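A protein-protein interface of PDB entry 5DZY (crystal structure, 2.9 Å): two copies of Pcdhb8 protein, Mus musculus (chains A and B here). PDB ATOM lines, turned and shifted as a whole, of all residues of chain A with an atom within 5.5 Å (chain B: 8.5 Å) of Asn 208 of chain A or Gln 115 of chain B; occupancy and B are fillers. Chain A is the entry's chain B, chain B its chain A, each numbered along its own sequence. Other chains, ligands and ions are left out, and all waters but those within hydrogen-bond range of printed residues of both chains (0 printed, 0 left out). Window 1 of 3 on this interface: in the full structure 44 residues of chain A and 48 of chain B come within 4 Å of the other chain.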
ATOM      1  N   ASP A 206     -22.627  -6.595  13.587  1.00  0.00           N
ATOM      2  CA  ASP A 206     -21.903  -7.858  13.550  1.00  0.00           C
ATOM      3  C   ASP A 206     -22.321  -8.796  14.675  1.00  0.00           C
ATOM      4  O   ASP A 206     -22.468  -8.383  15.825  1.00  0.00           O
ATOM      5  CB  ASP A 206     -20.395  -7.615  13.622  1.00  0.00           C
ATOM      6  CG  ASP A 206     -19.594  -8.901  13.537  1.00  0.00           C
ATOM      7  OD1 ASP A 206     -20.043  -9.841  12.846  1.00  0.00           O
ATOM      8  OD2 ASP A 206     -18.515  -8.972  14.162  1.00  0.00           O
ATOM      9  N   ILE A 207     -22.513 -10.063  14.327  1.00  0.00           N
ATOM     10  CA  ILE A 207     -22.777 -11.109  15.305  1.00  0.00           C
ATOM     11  C   ILE A 207     -21.776 -12.237  15.101  1.00  0.00           C
ATOM     12  O   ILE A 207     -21.491 -12.616  13.966  1.00  0.00           O
ATOM     13  CB  ILE A 207     -24.211 -11.662  15.188  1.00  0.00           C
ATOM     14  CG1 ILE A 207     -25.235 -10.538  15.347  1.00  0.00           C
ATOM     15  CG2 ILE A 207     -24.455 -12.743  16.229  1.00  0.00           C
ATOM     16  CD1 ILE A 207     -25.236  -9.908  16.720  1.00  0.00           C
ATOM     17  N   ASN A 208     -21.235 -12.763  16.194  1.00  0.00           N
ATOM     18  CA  ASN A 208     -20.287 -13.867  16.110  1.00  0.00           C
ATOM     19  C   ASN A 208     -20.957 -15.137  15.594  1.00  0.00           C
ATOM     20  O   ASN A 208     -21.382 -15.989  16.374  1.00  0.00           O
ATOM     21  CB  ASN A 208     -19.644 -14.129  17.472  1.00  0.00           C
ATOM     22  CG  ASN A 208     -18.490 -15.109  17.392  1.00  0.00           C
ATOM     23  OD1 ASN A 208     -18.012 -15.439  16.308  1.00  0.00           O
ATOM     24  ND2 ASN A 208     -18.032 -15.576  18.545  1.00  0.00           N
ATOM     25  N   ASP A 209     -21.052 -15.251  14.274  1.00  0.00           N
ATOM     26  CA  ASP A 209     -21.640 -16.428  13.647  1.00  0.00           C
ATOM     27  C   ASP A 209     -20.621 -17.126  12.754  1.00  0.00           C
ATOM     28  O   ASP A 209     -20.978 -17.923  11.889  1.00  0.00           O
ATOM     29  CB  ASP A 209     -22.889 -16.048  12.843  1.00  0.00           C
ATOM     30  CG  ASP A 209     -22.596 -15.044  11.741  1.00  0.00           C
ATOM     31  OD1 ASP A 209     -21.554 -14.360  11.810  1.00  0.00           O
ATOM     32  OD2 ASP A 209     -23.416 -14.934  10.804  1.00  0.00           O
ATOM     33  N   ASN A 210     -19.346 -16.817  12.973  1.00  0.00           N
ATOM     34  CA  ASN A 210     -18.261 -17.447  12.228  1.00  0.00           C
ATOM     35  C   ASN A 210     -17.223 -18.088  13.143  1.00  0.00           C
ATOM     36  O   ASN A 210     -16.774 -17.479  14.113  1.00  0.00           O
ATOM     37  CB  ASN A 210     -17.578 -16.429  11.312  1.00  0.00           C
ATOM     38  CG  ASN A 210     -18.440 -16.038  10.133  1.00  0.00           C
ATOM     39  OD1 ASN A 210     -18.393 -16.671   9.079  1.00  0.00           O
ATOM     40  ND2 ASN A 210     -19.234 -14.987  10.302  1.00  0.00           N
ATOM     41  N   ALA A 211     -16.847 -19.321  12.823  1.00  0.00           N
ATOM     42  CA  ALA A 211     -15.816 -20.029  13.570  1.00  0.00           C
ATOM     43  C   ALA A 211     -14.454 -19.828  12.912  1.00  0.00           C
ATOM     44  O   ALA A 211     -14.363 -19.742  11.687  1.00  0.00           O
ATOM     45  CB  ALA A 211     -16.151 -21.511  13.668  1.00  0.00           C
ATOM     46  N   ASP A 240     -10.600 -15.252  10.757  1.00  0.00           N
ATOM     47  CA  ASP A 240     -12.001 -15.191  11.153  1.00  0.00           C
ATOM     48  C   ASP A 240     -12.765 -14.238  10.237  1.00  0.00           C
ATOM     49  O   ASP A 240     -12.343 -13.101  10.019  1.00  0.00           O
ATOM     50  CB  ASP A 240     -12.130 -14.747  12.612  1.00  0.00           C
ATOM     51  CG  ASP A 240     -13.502 -15.035  13.196  1.00  0.00           C
ATOM     52  OD1 ASP A 240     -14.422 -15.389  12.429  1.00  0.00           O
ATOM     53  OD2 ASP A 240     -13.662 -14.903  14.428  1.00  0.00           O
ATOM     54  N   ASP A 242     -15.529 -12.851  10.807  1.00  0.00           N
ATOM     55  CA  ASP A 242     -16.120 -11.776  11.597  1.00  0.00           C
ATOM     56  C   ASP A 242     -15.152 -10.604  11.737  1.00  0.00           C
ATOM     57  O   ASP A 242     -14.065 -10.612  11.159  1.00  0.00           O
ATOM     58  CB  ASP A 242     -16.531 -12.286  12.980  1.00  0.00           C
ATOM     59  CG  ASP A 242     -17.632 -13.325  12.915  1.00  0.00           C
ATOM     60  OD1 ASP A 242     -18.426 -13.291  11.952  1.00  0.00           O
ATOM     61  OD2 ASP A 242     -17.705 -14.175  13.826  1.00  0.00           O
ATOM     62  N   HIS A 246     -15.131  -9.941  17.689  1.00  0.00           N
ATOM     63  CA  HIS A 246     -15.649 -11.222  17.227  1.00  0.00           C
ATOM     64  C   HIS A 246     -14.690 -11.860  16.228  1.00  0.00           C
ATOM     65  O   HIS A 246     -14.919 -12.974  15.757  1.00  0.00           O
ATOM     66  CB  HIS A 246     -17.030 -11.049  16.593  1.00  0.00           C
ATOM     67  CG  HIS A 246     -18.030 -10.386  17.488  1.00  0.00           C
ATOM     68  ND1 HIS A 246     -18.784 -11.081  18.408  1.00  0.00           N
ATOM     69  CD2 HIS A 246     -18.405  -9.089  17.599  1.00  0.00           C
ATOM     70  CE1 HIS A 246     -19.578 -10.242  19.050  1.00  0.00           C
ATOM     71  NE2 HIS A 246     -19.367  -9.026  18.577  1.00  0.00           N
ATOM     72  N   ASP A 294     -12.249 -17.902  19.374  1.00  0.00           N
ATOM     73  CA  ASP A 294     -12.580 -16.483  19.449  1.00  0.00           C
ATOM     74  C   ASP A 294     -13.078 -16.100  20.840  1.00  0.00           C
ATOM     75  O   ASP A 294     -12.805 -16.794  21.819  1.00  0.00           O
ATOM     76  CB  ASP A 294     -13.627 -16.113  18.390  1.00  0.00           C
ATOM     77  CG  ASP A 294     -14.837 -17.035  18.406  1.00  0.00           C
ATOM     78  OD1 ASP A 294     -15.215 -17.527  19.491  1.00  0.00           O
ATOM     79  OD2 ASP A 294     -15.417 -17.264  17.323  1.00  0.00           O
ATOM     80  N   SER A 295     -13.814 -14.996  20.919  1.00  0.00           N
ATOM     81  CA  SER A 295     -14.335 -14.519  22.194  1.00  0.00           C
ATOM     82  C   SER A 295     -15.770 -14.981  22.418  1.00  0.00           C
ATOM     83  O   SER A 295     -16.441 -14.523  23.343  1.00  0.00           O
ATOM     84  CB  SER A 295     -14.258 -12.992  22.262  1.00  0.00           C
ATOM     85  OG  SER A 295     -15.005 -12.398  21.214  1.00  0.00           O
ATOM     86  N   GLY A 296     -16.234 -15.894  21.572  1.00  0.00           N
ATOM     87  CA  GLY A 296     -17.599 -16.378  21.654  1.00  0.00           C
ATOM     88  C   GLY A 296     -17.712 -17.861  21.949  1.00  0.00           C
ATOM     89  O   GLY A 296     -18.752 -18.330  22.410  1.00  0.00           O
ATOM     90  N   GLY A 297     -16.642 -18.603  21.680  1.00  0.00           N
ATOM     91  CA  GLY A 297     -16.629 -20.030  21.943  1.00  0.00           C
ATOM     92  C   GLY A 297     -16.420 -20.873  20.702  1.00  0.00           C
ATOM     93  O   GLY A 297     -15.923 -21.997  20.787  1.00  0.00           O
ATOM     94  N   LEU A 298     -16.809 -20.335  19.550  1.00  0.00           N
ATOM     95  CA  LEU A 298     -16.596 -21.014  18.277  1.00  0.00           C
ATOM     96  C   LEU A 298     -15.108 -21.259  18.065  1.00  0.00           C
ATOM     97  O   LEU A 298     -14.285 -20.374  18.300  1.00  0.00           O
ATOM     98  CB  LEU A 298     -17.175 -20.198  17.121  1.00  0.00           C
ATOM     99  CG  LEU A 298     -18.694 -20.024  17.113  1.00  0.00           C
ATOM    100  CD1 LEU A 298     -19.133 -19.181  15.927  1.00  0.00           C
ATOM    101  CD2 LEU A 298     -19.389 -21.376  17.098  1.00  0.00           C
ATOM    102  N   LEU B 112     -14.004 -22.112  29.506  1.00  0.00           N
ATOM    103  CA  LEU B 112     -14.783 -22.110  28.274  1.00  0.00           C
ATOM    104  C   LEU B 112     -15.758 -20.940  28.251  1.00  0.00           C
ATOM    105  O   LEU B 112     -16.626 -20.826  29.115  1.00  0.00           O
ATOM    106  CB  LEU B 112     -15.544 -23.427  28.109  1.00  0.00           C
ATOM    107  CG  LEU B 112     -14.714 -24.672  27.792  1.00  0.00           C
ATOM    108  CD1 LEU B 112     -15.620 -25.875  27.581  1.00  0.00           C
ATOM    109  CD2 LEU B 112     -13.839 -24.436  26.571  1.00  0.00           C
ATOM    110  N   LYS B 113     -15.607 -20.067  27.260  1.00  0.00           N
ATOM    111  CA  LYS B 113     -16.506 -18.930  27.105  1.00  0.00           C
ATOM    112  C   LYS B 113     -17.431 -19.144  25.912  1.00  0.00           C
ATOM    113  O   LYS B 113     -17.100 -18.777  24.788  1.00  0.00           O
ATOM    114  CB  LYS B 113     -15.710 -17.634  26.938  1.00  0.00           C
ATOM    115  CG  LYS B 113     -14.832 -17.288  28.130  1.00  0.00           C
ATOM    116  CD  LYS B 113     -14.083 -15.984  27.906  1.00  0.00           C
ATOM    117  CE  LYS B 113     -13.217 -15.630  29.104  1.00  0.00           C
ATOM    118  NZ  LYS B 113     -12.484 -14.348  28.903  1.00  0.00           N
ATOM    119  N   ILE B 114     -18.593 -19.737  26.170  1.00  0.00           N
ATOM    120  CA  ILE B 114     -19.540 -20.072  25.111  1.00  0.00           C
ATOM    121  C   ILE B 114     -20.651 -19.028  24.987  1.00  0.00           C
ATOM    122  O   ILE B 114     -21.264 -18.641  25.982  1.00  0.00           O
ATOM    123  CB  ILE B 114     -20.171 -21.459  25.354  1.00  0.00           C
ATOM    124  CG1 ILE B 114     -19.079 -22.526  25.456  1.00  0.00           C
ATOM    125  CG2 ILE B 114     -21.160 -21.803  24.249  1.00  0.00           C
ATOM    126  CD1 ILE B 114     -19.603 -23.917  25.732  1.00  0.00           C
ATOM    127  N   GLN B 115     -20.902 -18.572  23.762  1.00  0.00           N
ATOM    128  CA  GLN B 115     -21.952 -17.591  23.509  1.00  0.00           C
ATOM    129  C   GLN B 115     -23.334 -18.204  23.722  1.00  0.00           C
ATOM    130  O   GLN B 115     -23.515 -19.415  23.603  1.00  0.00           O
ATOM    131  CB  GLN B 115     -21.832 -17.025  22.089  1.00  0.00           C
ATOM    132  CG  GLN B 115     -21.912 -18.067  20.986  1.00  0.00           C
ATOM    133  CD  GLN B 115     -21.543 -17.507  19.624  1.00  0.00           C
ATOM    134  OE1 GLN B 115     -21.020 -16.397  19.517  1.00  0.00           O
ATOM    135  NE2 GLN B 115     -21.815 -18.275  18.575  1.00  0.00           N
ATOM    136  N   GLU B 116     -24.305 -17.353  24.036  1.00  0.00           N
ATOM    137  CA  GLU B 116     -25.650 -17.794  24.400  1.00  0.00           C
ATOM    138  C   GLU B 116     -26.391 -18.480  23.252  1.00  0.00           C
ATOM    139  O   GLU B 116     -27.141 -19.430  23.471  1.00  0.00           O
ATOM    140  CB  GLU B 116     -26.467 -16.599  24.905  1.00  0.00           C
ATOM    141  CG  GLU B 116     -27.889 -16.914  25.332  1.00  0.00           C
ATOM    142  CD  GLU B 116     -28.656 -15.669  25.732  1.00  0.00           C
ATOM    143  OE1 GLU B 116     -28.083 -14.564  25.627  1.00  0.00           O
ATOM    144  OE2 GLU B 116     -29.825 -15.792  26.153  1.00  0.00           O
ATOM    145  N   ILE B 117     -26.173 -18.007  22.028  1.00  0.00           N
ATOM    146  CA  ILE B 117     -26.891 -18.536  20.867  1.00  0.00           C
ATOM    147  C   ILE B 117     -26.218 -19.754  20.241  1.00  0.00           C
ATOM    148  O   ILE B 117     -26.472 -20.078  19.080  1.00  0.00           O
ATOM    149  CB  ILE B 117     -27.056 -17.465  19.771  1.00  0.00           C
ATOM    150  CG1 ILE B 117     -25.698 -16.859  19.411  1.00  0.00           C
ATOM    151  CG2 ILE B 117     -28.030 -16.389  20.220  1.00  0.00           C
ATOM    152  CD1 ILE B 117     -25.769 -15.801  18.333  1.00  0.00           C
ATOM    153  N   ALA B 118     -25.365 -20.429  21.005  1.00  0.00           N
ATOM    154  CA  ALA B 118     -24.707 -21.638  20.521  1.00  0.00           C
ATOM    155  C   ALA B 118     -25.720 -22.764  20.337  1.00  0.00           C
ATOM    156  O   ALA B 118     -26.354 -23.201  21.297  1.00  0.00           O
ATOM    157  CB  ALA B 118     -23.606 -22.063  21.476  1.00  0.00           C
ATOM    158  N   GLN B 119     -25.872 -23.227  19.100  1.00  0.00           N
ATOM    159  CA  GLN B 119     -26.837 -24.275  18.788  1.00  0.00           C
ATOM    160  C   GLN B 119     -26.353 -25.645  19.251  1.00  0.00           C
ATOM    161  O   GLN B 119     -25.155 -25.924  19.221  1.00  0.00           O
ATOM    162  CB  GLN B 119     -27.129 -24.305  17.286  1.00  0.00           C
ATOM    163  CG  GLN B 119     -27.950 -23.125  16.792  1.00  0.00           C
ATOM    164  CD  GLN B 119     -28.348 -23.261  15.336  1.00  0.00           C
ATOM    165  OE1 GLN B 119     -27.810 -24.096  14.608  1.00  0.00           O
ATOM    166  NE2 GLN B 119     -29.301 -22.442  14.905  1.00  0.00           N
ATOM    167  N   THR B 122     -23.006 -28.531  18.870  1.00  0.00           N
ATOM    168  CA  THR B 122     -21.741 -27.821  18.735  1.00  0.00           C
ATOM    169  C   THR B 122     -20.677 -28.450  19.626  1.00  0.00           C
ATOM    170  O   THR B 122     -20.896 -28.655  20.821  1.00  0.00           O
ATOM    171  CB  THR B 122     -21.888 -26.329  19.092  1.00  0.00           C
ATOM    172  OG1 THR B 122     -22.922 -25.741  18.293  1.00  0.00           O
ATOM    173  CG2 THR B 122     -20.581 -25.589  18.844  1.00  0.00           C
ATOM    174  N   PHE B 124     -16.925 -28.671  21.519  1.00  0.00           N
ATOM    175  CA  PHE B 124     -15.944 -27.816  22.172  1.00  0.00           C
ATOM    176  C   PHE B 124     -14.759 -28.648  22.649  1.00  0.00           C
ATOM    177  O   PHE B 124     -14.919 -29.549  23.472  1.00  0.00           O
ATOM    178  CB  PHE B 124     -16.574 -27.063  23.345  1.00  0.00           C
ATOM    179  CG  PHE B 124     -17.679 -26.129  22.941  1.00  0.00           C
ATOM    180  CD1 PHE B 124     -17.399 -24.828  22.559  1.00  0.00           C
ATOM    181  CD2 PHE B 124     -18.998 -26.552  22.943  1.00  0.00           C
ATOM    182  CE1 PHE B 124     -18.411 -23.966  22.187  1.00  0.00           C
ATOM    183  CE2 PHE B 124     -20.015 -25.696  22.571  1.00  0.00           C
ATOM    184  CZ  PHE B 124     -19.721 -24.401  22.192  1.00  0.00           C
ATOM    185  N   PHE B 150     -24.750 -30.195  28.768  1.00  0.00           N
ATOM    186  CA  PHE B 150     -23.637 -30.793  28.037  1.00  0.00           C
ATOM    187  C   PHE B 150     -23.480 -32.293  28.273  1.00  0.00           C
ATOM    188  O   PHE B 150     -24.056 -32.856  29.204  1.00  0.00           O
ATOM    189  CB  PHE B 150     -22.329 -30.090  28.410  1.00  0.00           C
ATOM    190  CG  PHE B 150     -22.267 -28.651  27.988  1.00  0.00           C
ATOM    191  CD1 PHE B 150     -22.711 -27.648  28.831  1.00  0.00           C
ATOM    192  CD2 PHE B 150     -21.752 -28.301  26.751  1.00  0.00           C
ATOM    193  CE1 PHE B 150     -22.653 -26.322  28.445  1.00  0.00           C
ATOM    194  CE2 PHE B 150     -21.687 -26.977  26.361  1.00  0.00           C
ATOM    195  CZ  PHE B 150     -22.139 -25.986  27.209  1.00  0.00           C
ATOM    196  N   LEU B 168     -22.763 -29.904  23.277  1.00  0.00           N
ATOM    197  CA  LEU B 168     -23.957 -29.239  23.784  1.00  0.00           C
ATOM    198  C   LEU B 168     -25.222 -29.969  23.338  1.00  0.00           C
ATOM    199  O   LEU B 168     -25.310 -30.435  22.203  1.00  0.00           O
ATOM    200  CB  LEU B 168     -23.992 -27.783  23.315  1.00  0.00           C
ATOM    201  CG  LEU B 168     -25.128 -26.907  23.841  1.00  0.00           C
ATOM    202  CD1 LEU B 168     -25.062 -26.804  25.353  1.00  0.00           C
ATOM    203  CD2 LEU B 168     -25.073 -25.528  23.205  1.00  0.00           C
ATOM    204  N   ALA B 171     -29.675 -25.614  24.446  1.00  0.00           N
ATOM    205  CA  ALA B 171     -29.158 -24.254  24.307  1.00  0.00           C
ATOM    206  C   ALA B 171     -29.055 -23.523  25.643  1.00  0.00           C
ATOM    207  O   ALA B 171     -29.879 -23.718  26.538  1.00  0.00           O
ATOM    208  CB  ALA B 171     -30.029 -23.463  23.344  1.00  0.00           C
ATOM    209  N   LEU B 172     -28.036 -22.678  25.765  1.00  0.00           N
ATOM    210  CA  LEU B 172     -27.789 -21.934  26.996  1.00  0.00           C
ATOM    211  C   LEU B 172     -28.628 -20.663  27.068  1.00  0.00           C
ATOM    212  O   LEU B 172     -29.293 -20.289  26.102  1.00  0.00           O
ATOM    213  CB  LEU B 172     -26.306 -21.582  27.116  1.00  0.00           C
ATOM    214  CG  LEU B 172     -25.312 -22.744  27.139  1.00  0.00           C
ATOM    215  CD1 LEU B 172     -23.885 -22.222  27.166  1.00  0.00           C
ATOM    216  CD2 LEU B 172     -25.578 -23.652  28.329  1.00  0.00           C
ATOM    217  N   ASP B 173     -28.583 -20.003  28.221  1.00  0.00           N
ATOM    218  CA  ASP B 173     -29.296 -18.748  28.426  1.00  0.00           C
ATOM    219  C   ASP B 173     -28.714 -18.001  29.621  1.00  0.00           C
ATOM    220  O   ASP B 173     -28.842 -18.447  30.763  1.00  0.00           O
ATOM    221  CB  ASP B 173     -30.791 -19.001  28.633  1.00  0.00           C
ATOM    222  CG  ASP B 173     -31.604 -17.721  28.642  1.00  0.00           C
ATOM    223  OD1 ASP B 173     -32.045 -17.290  27.557  1.00  0.00           O
ATOM    224  OD2 ASP B 173     -31.803 -17.149  29.734  1.00  0.00           O
ATOM    225  N   ARG B 174     -28.071 -16.867  29.357  1.00  0.00           N
ATOM    226  CA  ARG B 174     -27.437 -16.084  30.411  1.00  0.00           C
ATOM    227  C   ARG B 174     -28.473 -15.470  31.348  1.00  0.00           C
ATOM    228  O   ARG B 174     -28.200 -15.230  32.524  1.00  0.00           O
ATOM    229  CB  ARG B 174     -26.561 -14.982  29.812  1.00  0.00           C
ATOM    230  CG  ARG B 174     -25.681 -14.279  30.833  1.00  0.00           C
ATOM    231  CD  ARG B 174     -25.133 -12.975  30.291  1.00  0.00           C
ATOM    232  NE  ARG B 174     -26.200 -12.031  29.975  1.00  0.00           N
ATOM    233  CZ  ARG B 174     -26.746 -11.199  30.856  1.00  0.00           C
ATOM    234  NH1 ARG B 174     -27.713 -10.374  30.479  1.00  0.00           N
ATOM    235  NH2 ARG B 174     -26.325 -11.193  32.113  1.00  0.00           N
ATOM    236  N   ILE B 202     -17.508 -22.978  32.612  1.00  0.00           N
ATOM    237  CA  ILE B 202     -18.183 -22.458  31.428  1.00  0.00           C
ATOM    238  C   ILE B 202     -18.785 -21.080  31.685  1.00  0.00           C
ATOM    239  O   ILE B 202     -19.670 -20.923  32.524  1.00  0.00           O
ATOM    240  CB  ILE B 202     -19.293 -23.412  30.955  1.00  0.00           C
ATOM    241  CG1 ILE B 202     -18.721 -24.808  30.707  1.00  0.00           C
ATOM    242  CG2 ILE B 202     -19.962 -22.872  29.701  1.00  0.00           C
ATOM    243  CD1 ILE B 202     -19.760 -25.835  30.325  1.00  0.00           C
ATOM    244  N   GLU B 203     -18.296 -20.084  30.953  1.00  0.00           N
ATOM    245  CA  GLU B 203     -18.797 -18.720  31.082  1.00  0.00           C
ATOM    246  C   GLU B 203     -19.675 -18.351  29.892  1.00  0.00           C
ATOM    247  O   GLU B 203     -19.191 -18.236  28.766  1.00  0.00           O
ATOM    248  CB  GLU B 203     -17.636 -17.733  31.210  1.00  0.00           C
ATOM    249  CG  GLU B 203     -18.064 -16.278  31.305  1.00  0.00           C
ATOM    250  CD  GLU B 203     -16.885 -15.334  31.420  1.00  0.00           C
ATOM    251  OE1 GLU B 203     -15.736 -15.819  31.476  1.00  0.00           O
ATOM    252  OE2 GLU B 203     -17.108 -14.104  31.452  1.00  0.00           O
ATOM    253  N   VAL B 204     -20.966 -18.166  30.144  1.00  0.00           N
ATOM    254  CA  VAL B 204     -21.913 -17.854  29.079  1.00  0.00           C
ATOM    255  C   VAL B 204     -21.821 -16.391  28.651  1.00  0.00           C
ATOM    256  O   VAL B 204     -22.177 -15.488  29.409  1.00  0.00           O
ATOM    257  CB  VAL B 204     -23.361 -18.163  29.503  1.00  0.00           C
ATOM    258  CG1 VAL B 204     -24.326 -17.816  28.379  1.00  0.00           C
ATOM    259  CG2 VAL B 204     -23.497 -19.624  29.896  1.00  0.00           C
ATOM    260  N   VAL B 205     -21.341 -16.168  27.431  1.00  0.00           N
ATOM    261  CA  VAL B 205     -21.218 -14.822  26.885  1.00  0.00           C
ATOM    262  C   VAL B 205     -22.593 -14.266  26.520  1.00  0.00           C
ATOM    263  O   VAL B 205     -23.397 -14.950  25.893  1.00  0.00           O
ATOM    264  CB  VAL B 205     -20.311 -14.800  25.640  1.00  0.00           C
ATOM    265  CG1 VAL B 205     -20.187 -13.384  25.093  1.00  0.00           C
ATOM    266  CG2 VAL B 205     -18.941 -15.369  25.972  1.00  0.00           C
ATOM    267  N   ASP B 206     -22.855 -13.025  26.915  1.00  0.00           N
ATOM    268  CA  ASP B 206     -24.144 -12.392  26.660  1.00  0.00           C
ATOM    269  C   ASP B 206     -24.400 -12.154  25.176  1.00  0.00           C
ATOM    270  O   ASP B 206     -23.537 -11.655  24.456  1.00  0.00           O
ATOM    271  CB  ASP B 206     -24.240 -11.061  27.408  1.00  0.00           C
ATOM    272  CG  ASP B 206     -25.569 -10.361  27.183  1.00  0.00           C
ATOM    273  OD1 ASP B 206     -26.587 -11.063  27.004  1.00  0.00           O
ATOM    274  OD2 ASP B 206     -25.596  -9.112  27.185  1.00  0.00           O
ATOM    275  N   ILE B 207     -25.598 -12.511  24.727  1.00  0.00           N
ATOM    276  CA  ILE B 207     -26.031 -12.213  23.365  1.00  0.00           C
ATOM    277  C   ILE B 207     -27.333 -11.413  23.408  1.00  0.00           C
ATOM    278  O   ILE B 207     -28.244 -11.743  24.169  1.00  0.00           O
ATOM    279  CB  ILE B 207     -26.230 -13.496  22.528  1.00  0.00           C
ATOM    280  CG1 ILE B 207     -24.938 -14.316  22.493  1.00  0.00           C
ATOM    281  CG2 ILE B 207     -26.665 -13.153  21.112  1.00  0.00           C
ATOM    282  CD1 ILE B 207     -23.786 -13.611  21.809  1.00  0.00           C
ATOM    283  N   HIS B 246     -25.237  -4.521  25.020  1.00  0.00           N
ATOM    284  CA  HIS B 246     -26.425  -5.184  24.493  1.00  0.00           C
ATOM    285  C   HIS B 246     -27.678  -4.814  25.287  1.00  0.00           C
ATOM    286  O   HIS B 246     -28.795  -5.133  24.883  1.00  0.00           O
ATOM    287  CB  HIS B 246     -26.234  -6.704  24.497  1.00  0.00           C
ATOM    288  CG  HIS B 246     -25.046  -7.168  23.714  1.00  0.00           C
ATOM    289  ND1 HIS B 246     -25.154  -7.735  22.462  1.00  0.00           N
ATOM    290  CD2 HIS B 246     -23.724  -7.153  24.005  1.00  0.00           C
ATOM    291  CE1 HIS B 246     -23.951  -8.048  22.016  1.00  0.00           C
ATOM    292  NE2 HIS B 246     -23.064  -7.705  22.933  1.00  0.00           N
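Among the printed residues, pairs that only touch across the chains: Gly 296 of chain A with Ile 114 of chain B (3.3 Å), Gly 297 of chain A with Phe 124 of chain B (3.5 Å), Ser 295 of chain A with Val 205 of chain B (3.7 Å), Leu 298 of chain A with Gln 115 of chain B (3.9 Å) and Ile 207 of chain A with Ile 117 of chain B (3.9 Å).
Of the printed residues of chain B, Ile 207 of chain A touches Ile 117.
Of the printed residues of chain A, Lys 113 of chain B touches Gly 296 and Gly 297.
Of the printed residues of chain B, Leu 298 of chain A touches Gln 115.
Printed residues of chain A within 4 Å of Val 205 of chain B: Ser 295.
Printed residues of chain B within 4 Å of Gly 297 of chain A: Lys 113 and Phe 124.
The nearest residue of chain A that does not touch Gln 115 of chain B is Gly 297 of chain A (4.7 Å).
Printed residues of chain B that touch a printed residue of chain A: Lys 113, Ile 114, Gln 115, Ile 117, Phe 124 and Val 205.
Hydrophobic or aromatic side chains of chain A that line the printed part of chain B: Ile 207 and Leu 298.
The backbone carbonyl oxygen of Lys 113 of chain B sits close to the backbone carbonyl oxygen of Gly 296 of chain A (2.9 Å).
O of Asn 208 of chain A lies close to OE1 of Gln 115 of chain B (3.2 Å).
The backbone NH (N) of Gly 297 of chain A sits close to the backbone carbonyl oxygen (O) of Lys 113 of chain B.
O of Gly 296 of chain A is in hydrogen-bond range of N of Gln 115 of chain B (2.6 Å).
Positions printed for both chains: 206, 207 and 246.
The backbone NH (N) of Ile 114 of chain B lies within hydrogen-bond range of the backbone carbonyl oxygen (O) of Glu 203 of chain B (3.1 Å).
O of Ile 114 of chain B sits at hydrogen-bond distance from N of Val 205 of chain B (2.9 Å).
OD1 of Asp 294 of chain A sits at hydrogen-bond distance from N of Gly 297 of chain A.
The side-chain carboxylate (OD1) of Asp 294 of chain A sits at hydrogen-bond distance from the backbone NH (N) of Leu 298 of chain A, at 3.2 Å.
OD1 of Asp 294 of chain A sits at hydrogen-bond distance from N of Gly 296 of chain A, 2.8 Å away.
O of Val 205 of chain B lies within hydrogen-bond range of N of Glu 116 of chain B (3.2 Å).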
